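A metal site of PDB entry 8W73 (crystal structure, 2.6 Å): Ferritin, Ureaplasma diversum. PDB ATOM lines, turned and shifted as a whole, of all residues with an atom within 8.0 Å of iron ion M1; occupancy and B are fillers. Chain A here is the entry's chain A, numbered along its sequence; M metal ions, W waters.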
ATOM      1  N   ASN A  27      -3.414  -4.677  -5.671  1.00  0.00           N
ATOM      2  CA  ASN A  27      -2.538  -5.595  -6.413  1.00  0.00           C
ATOM      3  C   ASN A  27      -2.073  -6.743  -5.552  1.00  0.00           C
ATOM      4  O   ASN A  27      -1.964  -7.882  -6.020  1.00  0.00           O
ATOM      5  CB  ASN A  27      -1.348  -4.827  -6.979  1.00  0.00           C
ATOM      6  CG  ASN A  27      -1.675  -4.179  -8.311  1.00  0.00           C
ATOM      7  OD1 ASN A  27      -1.710  -4.866  -9.331  1.00  0.00           O
ATOM      8  ND2 ASN A  27      -1.959  -2.885  -8.304  1.00  0.00           N
ATOM      9  N   HIS A  56       1.283 -16.544 -13.589  1.00  0.00           N
ATOM     10  CA  HIS A  56       2.081 -15.442 -14.112  1.00  0.00           C
ATOM     11  C   HIS A  56       1.432 -14.098 -13.826  1.00  0.00           C
ATOM     12  O   HIS A  56       2.119 -13.117 -13.527  1.00  0.00           O
ATOM     13  CB  HIS A  56       2.312 -15.617 -15.621  1.00  0.00           C
ATOM     14  CG  HIS A  56       3.174 -16.782 -15.979  1.00  0.00           C
ATOM     15  ND1 HIS A  56       4.055 -17.365 -15.101  1.00  0.00           N
ATOM     16  CD2 HIS A  56       3.271 -17.494 -17.124  1.00  0.00           C
ATOM     17  CE1 HIS A  56       4.664 -18.380 -15.682  1.00  0.00           C
ATOM     18  NE2 HIS A  56       4.204 -18.475 -16.916  1.00  0.00           N
ATOM     19  N   LEU A  57       0.098 -14.036 -13.915  1.00  0.00           N
ATOM     20  CA  LEU A  57      -0.594 -12.805 -13.559  1.00  0.00           C
ATOM     21  C   LEU A  57      -0.502 -12.560 -12.055  1.00  0.00           C
ATOM     22  O   LEU A  57      -0.339 -11.409 -11.610  1.00  0.00           O
ATOM     23  CB  LEU A  57      -2.059 -12.892 -14.020  1.00  0.00           C
ATOM     24  CG  LEU A  57      -2.928 -11.625 -14.106  1.00  0.00           C
ATOM     25  CD1 LEU A  57      -2.303 -10.520 -14.939  1.00  0.00           C
ATOM     26  CD2 LEU A  57      -4.306 -11.975 -14.635  1.00  0.00           C
ATOM     27  N   GLU A  59       2.028 -13.432 -10.066  1.00  0.00           N
ATOM     28  CA  GLU A  59       3.360 -12.931  -9.748  1.00  0.00           C
ATOM     29  C   GLU A  59       3.552 -11.514 -10.266  1.00  0.00           C
ATOM     30  O   GLU A  59       4.334 -10.744  -9.697  1.00  0.00           O
ATOM     31  CB  GLU A  59       4.412 -13.857 -10.314  1.00  0.00           C
ATOM     32  CG  GLU A  59       4.387 -15.197  -9.610  1.00  0.00           C
ATOM     33  CD  GLU A  59       5.014 -16.303 -10.426  1.00  0.00           C
ATOM     34  OE1 GLU A  59       5.174 -17.408  -9.871  1.00  0.00           O
ATOM     35  OE2 GLU A  59       5.334 -16.065 -11.617  1.00  0.00           O
ATOM     36  N   ASP A  60       2.837 -11.165 -11.325  1.00  0.00           N
ATOM     37  CA  ASP A  60       2.828  -9.808 -11.836  1.00  0.00           C
ATOM     38  C   ASP A  60       2.214  -8.843 -10.817  1.00  0.00           C
ATOM     39  O   ASP A  60       2.860  -7.876 -10.399  1.00  0.00           O
ATOM     40  CB  ASP A  60       2.082  -9.797 -13.168  1.00  0.00           C
ATOM     41  CG  ASP A  60       2.355  -8.584 -13.981  1.00  0.00           C
ATOM     42  OD1 ASP A  60       3.512  -8.120 -13.985  1.00  0.00           O
ATOM     43  OD2 ASP A  60       1.387  -8.104 -14.627  1.00  0.00           O
ATOM     44  N   LYS A  61       0.977  -9.121 -10.383  1.00  0.00           N
ATOM     45  CA  LYS A  61       0.298  -8.247  -9.433  1.00  0.00           C
ATOM     46  C   LYS A  61       1.111  -8.069  -8.153  1.00  0.00           C
ATOM     47  O   LYS A  61       1.237  -6.961  -7.641  1.00  0.00           O
ATOM     48  CB  LYS A  61      -1.100  -8.790  -9.083  1.00  0.00           C
ATOM     49  CG  LYS A  61      -2.093  -8.917 -10.255  1.00  0.00           C
ATOM     50  CD  LYS A  61      -2.226  -7.621 -11.026  1.00  0.00           C
ATOM     51  CE  LYS A  61      -3.213  -7.770 -12.174  1.00  0.00           C
ATOM     52  NZ  LYS A  61      -3.305  -6.540 -13.020  1.00  0.00           N
ATOM     53  N   VAL A  64       5.919  -6.377  -9.835  1.00  0.00           N
ATOM     54  CA  VAL A  64       6.233  -5.010 -10.226  1.00  0.00           C
ATOM     55  C   VAL A  64       5.052  -4.092  -9.972  1.00  0.00           C
ATOM     56  O   VAL A  64       5.230  -2.902  -9.673  1.00  0.00           O
ATOM     57  CB  VAL A  64       6.679  -4.946 -11.702  1.00  0.00           C
ATOM     58  CG1 VAL A  64       8.077  -5.531 -11.861  1.00  0.00           C
ATOM     59  CG2 VAL A  64       5.677  -5.645 -12.609  1.00  0.00           C
ATOM     60  N   HIS A  65       3.829  -4.611 -10.080  1.00  0.00           N
ATOM     61  CA  HIS A  65       2.659  -3.783  -9.822  1.00  0.00           C
ATOM     62  C   HIS A  65       2.722  -3.172  -8.428  1.00  0.00           C
ATOM     63  O   HIS A  65       2.391  -1.988  -8.239  1.00  0.00           O
ATOM     64  CB  HIS A  65       1.387  -4.605 -10.007  1.00  0.00           C
ATOM     65  CG  HIS A  65       0.969  -4.748 -11.428  1.00  0.00           C
ATOM     66  ND1 HIS A  65      -0.164  -4.145 -11.946  1.00  0.00           N
ATOM     67  CD2 HIS A  65       1.528  -5.432 -12.467  1.00  0.00           C
ATOM     68  CE1 HIS A  65      -0.281  -4.447 -13.226  1.00  0.00           C
ATOM     69  NE2 HIS A  65       0.729  -5.223 -13.569  1.00  0.00           N
ATOM     70  N   GLU A 106      -9.788  -7.528 -13.749  1.00  0.00           N
ATOM     71  CA  GLU A 106      -8.834  -6.726 -14.521  1.00  0.00           C
ATOM     72  C   GLU A 106      -9.526  -5.511 -15.137  1.00  0.00           C
ATOM     73  O   GLU A 106      -8.914  -4.443 -15.277  1.00  0.00           O
ATOM     74  CB  GLU A 106      -8.191  -7.568 -15.628  1.00  0.00           C
ATOM     75  CG  GLU A 106      -7.306  -8.663 -15.098  1.00  0.00           C
ATOM     76  CD  GLU A 106      -6.181  -8.113 -14.261  1.00  0.00           C
ATOM     77  OE1 GLU A 106      -5.506  -7.175 -14.704  1.00  0.00           O
ATOM     78  OE2 GLU A 106      -5.992  -8.623 -13.162  1.00  0.00           O
ATOM     79  N   VAL A 109      -9.574  -2.952 -12.609  1.00  0.00           N
ATOM     80  CA  VAL A 109      -8.257  -2.331 -12.426  1.00  0.00           C
ATOM     81  C   VAL A 109      -8.111  -1.132 -13.353  1.00  0.00           C
ATOM     82  O   VAL A 109      -7.645  -0.055 -12.949  1.00  0.00           O
ATOM     83  CB  VAL A 109      -7.141  -3.358 -12.636  1.00  0.00           C
ATOM     84  CG1 VAL A 109      -5.817  -2.654 -12.896  1.00  0.00           C
ATOM     85  CG2 VAL A 109      -7.039  -4.264 -11.406  1.00  0.00           C
ATOM     86  N   TRP A 134       2.513   3.982 -16.848  1.00  0.00           N
ATOM     87  CA  TRP A 134       2.766   2.560 -17.005  1.00  0.00           C
ATOM     88  C   TRP A 134       1.508   1.754 -16.707  1.00  0.00           C
ATOM     89  O   TRP A 134       1.177   0.816 -17.428  1.00  0.00           O
ATOM     90  CB  TRP A 134       3.904   2.124 -16.087  1.00  0.00           C
ATOM     91  CG  TRP A 134       4.295   0.709 -16.318  1.00  0.00           C
ATOM     92  CD1 TRP A 134       5.191   0.244 -17.247  1.00  0.00           C
ATOM     93  CD2 TRP A 134       3.775  -0.442 -15.635  1.00  0.00           C
ATOM     94  NE1 TRP A 134       5.284  -1.136 -17.152  1.00  0.00           N
ATOM     95  CE2 TRP A 134       4.424  -1.580 -16.182  1.00  0.00           C
ATOM     96  CE3 TRP A 134       2.838  -0.625 -14.606  1.00  0.00           C
ATOM     97  CZ2 TRP A 134       4.171  -2.879 -15.720  1.00  0.00           C
ATOM     98  CZ3 TRP A 134       2.588  -1.938 -14.148  1.00  0.00           C
ATOM     99  CH2 TRP A 134       3.257  -3.035 -14.715  1.00  0.00           C
ATOM    100  N   TYR A 135       0.776   2.160 -15.666  1.00  0.00           N
ATOM    101  CA  TYR A 135      -0.394   1.405 -15.254  1.00  0.00           C
ATOM    102  C   TYR A 135      -1.558   1.585 -16.217  1.00  0.00           C
ATOM    103  O   TYR A 135      -2.388   0.683 -16.351  1.00  0.00           O
ATOM    104  CB  TYR A 135      -0.833   1.832 -13.851  1.00  0.00           C
ATOM    105  CG  TYR A 135       0.136   1.408 -12.791  1.00  0.00           C
ATOM    106  CD1 TYR A 135       1.289   2.131 -12.560  1.00  0.00           C
ATOM    107  CD2 TYR A 135      -0.083   0.260 -12.033  1.00  0.00           C
ATOM    108  CE1 TYR A 135       2.194   1.741 -11.580  1.00  0.00           C
ATOM    109  CE2 TYR A 135       0.800  -0.131 -11.066  1.00  0.00           C
ATOM    110  CZ  TYR A 135       1.939   0.607 -10.843  1.00  0.00           C
ATOM    111  OH  TYR A 135       2.837   0.201  -9.867  1.00  0.00           O
ATOM    112  N   ARG A 137      -1.413   1.647 -19.547  1.00  0.00           N
ATOM    113  CA  ARG A 137      -1.264   0.649 -20.557  1.00  0.00           C
ATOM    114  C   ARG A 137      -1.229  -0.787 -20.093  1.00  0.00           C
ATOM    115  O   ARG A 137      -1.639  -1.647 -20.827  1.00  0.00           O
ATOM    116  CB  ARG A 137      -0.061   0.962 -21.456  1.00  0.00           C
ATOM    117  CG  ARG A 137       1.252   1.192 -20.752  1.00  0.00           C
ATOM    118  CD  ARG A 137       2.238   0.052 -20.978  1.00  0.00           C
ATOM    119  NE  ARG A 137       2.751   0.029 -22.345  1.00  0.00           N
ATOM    120  CZ  ARG A 137       4.039   0.111 -22.669  1.00  0.00           C
ATOM    121  NH1 ARG A 137       4.417   0.075 -23.935  1.00  0.00           N
ATOM    122  NH2 ARG A 137       4.950   0.227 -21.713  1.00  0.00           N
ATOM    123  N   ASP A 138      -0.758  -1.068 -18.905  1.00  0.00           N
ATOM    124  CA  ASP A 138      -0.785  -2.412 -18.438  1.00  0.00           C
ATOM    125  C   ASP A 138      -2.195  -2.761 -18.092  1.00  0.00           C
ATOM    126  O   ASP A 138      -2.525  -3.923 -18.063  1.00  0.00           O
ATOM    127  CB  ASP A 138       0.130  -2.660 -17.250  1.00  0.00           C
ATOM    128  CG  ASP A 138       0.829  -3.984 -17.315  1.00  0.00           C
ATOM    129  OD1 ASP A 138       1.646  -4.146 -18.233  1.00  0.00           O
ATOM    130  OD2 ASP A 138       0.600  -4.837 -16.445  1.00  0.00           O
ATOM    131  N   GLY A 139      -3.032  -1.773 -17.830  1.00  0.00           N
ATOM    132  CA  GLY A 139      -4.431  -2.114 -17.601  1.00  0.00           C
ATOM    133  C   GLY A 139      -5.044  -2.753 -18.834  1.00  0.00           C
ATOM    134  O   GLY A 139      -5.718  -3.787 -18.750  1.00  0.00           O
ATOM    135  N   LYS A 141      -3.251  -4.013 -21.427  1.00  0.00           N
ATOM    136  CA  LYS A 141      -2.485  -5.184 -21.856  1.00  0.00           C
ATOM    137  C   LYS A 141      -2.887  -6.419 -21.063  1.00  0.00           C
ATOM    138  O   LYS A 141      -3.197  -7.461 -21.646  1.00  0.00           O
ATOM    139  CB  LYS A 141      -0.985  -4.927 -21.736  1.00  0.00           C
ATOM    140  CG  LYS A 141      -0.154  -6.096 -22.276  1.00  0.00           C
ATOM    141  CD  LYS A 141       1.051  -6.389 -21.409  1.00  0.00           C
ATOM    142  CE  LYS A 141       0.616  -6.691 -19.985  1.00  0.00           C
ATOM    143  NZ  LYS A 141       1.559  -7.577 -19.235  1.00  0.00           N
ATOM    144  N   ASP A 142      -2.864  -6.325 -19.733  1.00  0.00           N
ATOM    145  CA  ASP A 142      -3.257  -7.455 -18.905  1.00  0.00           C
ATOM    146  C   ASP A 142      -4.691  -7.869 -19.209  1.00  0.00           C
ATOM    147  O   ASP A 142      -5.005  -9.068 -19.251  1.00  0.00           O
ATOM    148  CB  ASP A 142      -3.108  -7.106 -17.409  1.00  0.00           C
ATOM    149  CG  ASP A 142      -1.666  -7.220 -16.897  1.00  0.00           C
ATOM    150  OD1 ASP A 142      -0.796  -7.789 -17.601  1.00  0.00           O
ATOM    151  OD2 ASP A 142      -1.391  -6.749 -15.766  1.00  0.00           O
ATOM    152  N   LEU A 143      -5.580  -6.901 -19.419  1.00  0.00           N
ATOM    153  CA  LEU A 143      -6.965  -7.252 -19.697  1.00  0.00           C
ATOM    154  C   LEU A 143      -7.079  -7.947 -21.049  1.00  0.00           C
ATOM    155  O   LEU A 143      -7.872  -8.878 -21.211  1.00  0.00           O
ATOM    156  CB  LEU A 143      -7.851  -6.013 -19.655  1.00  0.00           C
ATOM    157  CG  LEU A 143      -9.298  -6.295 -20.054  1.00  0.00           C
ATOM    158  CD1 LEU A 143     -10.131  -6.530 -18.831  1.00  0.00           C
ATOM    159  CD2 LEU A 143      -9.881  -5.164 -20.891  1.00  0.00           C
ATOM    160  N   GLU A 145      -4.696  -9.751 -22.496  1.00  0.00           N
ATOM    161  CA  GLU A 145      -4.135 -11.090 -22.335  1.00  0.00           C
ATOM    162  C   GLU A 145      -5.169 -12.037 -21.741  1.00  0.00           C
ATOM    163  O   GLU A 145      -5.329 -13.169 -22.219  1.00  0.00           O
ATOM    164  CB  GLU A 145      -2.883 -11.046 -21.454  1.00  0.00           C
ATOM    165  CG  GLU A 145      -1.652 -10.485 -22.133  1.00  0.00           C
ATOM    166  CD  GLU A 145      -0.428 -10.487 -21.217  1.00  0.00           C
ATOM    167  OE1 GLU A 145       0.666 -10.139 -21.710  1.00  0.00           O
ATOM    168  OE2 GLU A 145      -0.558 -10.837 -20.021  1.00  0.00           O
HETATM  169 FE    FE M   1       0.660  -6.386 -15.461  1.00  0.00          FE
HETATM  170 FE    FE M   2       3.097 -11.010 -18.941  1.00  0.00          FE
HETATM  171  O   HOH W   1       3.044  -6.378 -16.321  1.00  0.00           O
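The side-chain amino group of Lys 141 lies within salt-bridge range of the side-chain carboxylate of Asp 142 (2.9 Å). The backbone carbonyl oxygen (O) of His 65 is in hydrogen-bond range of the side-chain hydroxyl (OH) of Tyr 135 (2.8 Å). The side-chain amino group (NZ) of Lys 61 lies close to the side-chain carboxylate (OD2) of Asp 142, at 3.4 Å. The side-chain carboxylate of Asp 138 lies within salt-bridge range of the side-chain amino group of Lys 141, 3.6 Å away. A ring nitrogen (ND1) of His 65 lies within hydrogen-bond range of the side-chain amide oxygen (OD1) of Asn 27, at 3.1 Å.
Of the 19 residues printed, 4 come within 4 Å of iron ion M1. The nearest printed residue that does not touch iron ion M1 is Lys 141 (4.1 Å).
OD2 of Asp 138 is bound to iron ion M1 (1.8 Å). The side-chain carboxylate (OD2) of Asp 60 is bound to iron ion M1 (2.0 Å). Iron ion M1 is bound by OD2 of Asp 142 (2.1 Å). NE2 of His 65 binds iron ion M1 (2.2 Å). Iron ion M1 is bound by water W1, 2.5 Å away.
Water W1 lies within hydrogen-bond range of OD1 of Asp 60, OD1 of Asp 138 and NZ of Lys 141.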
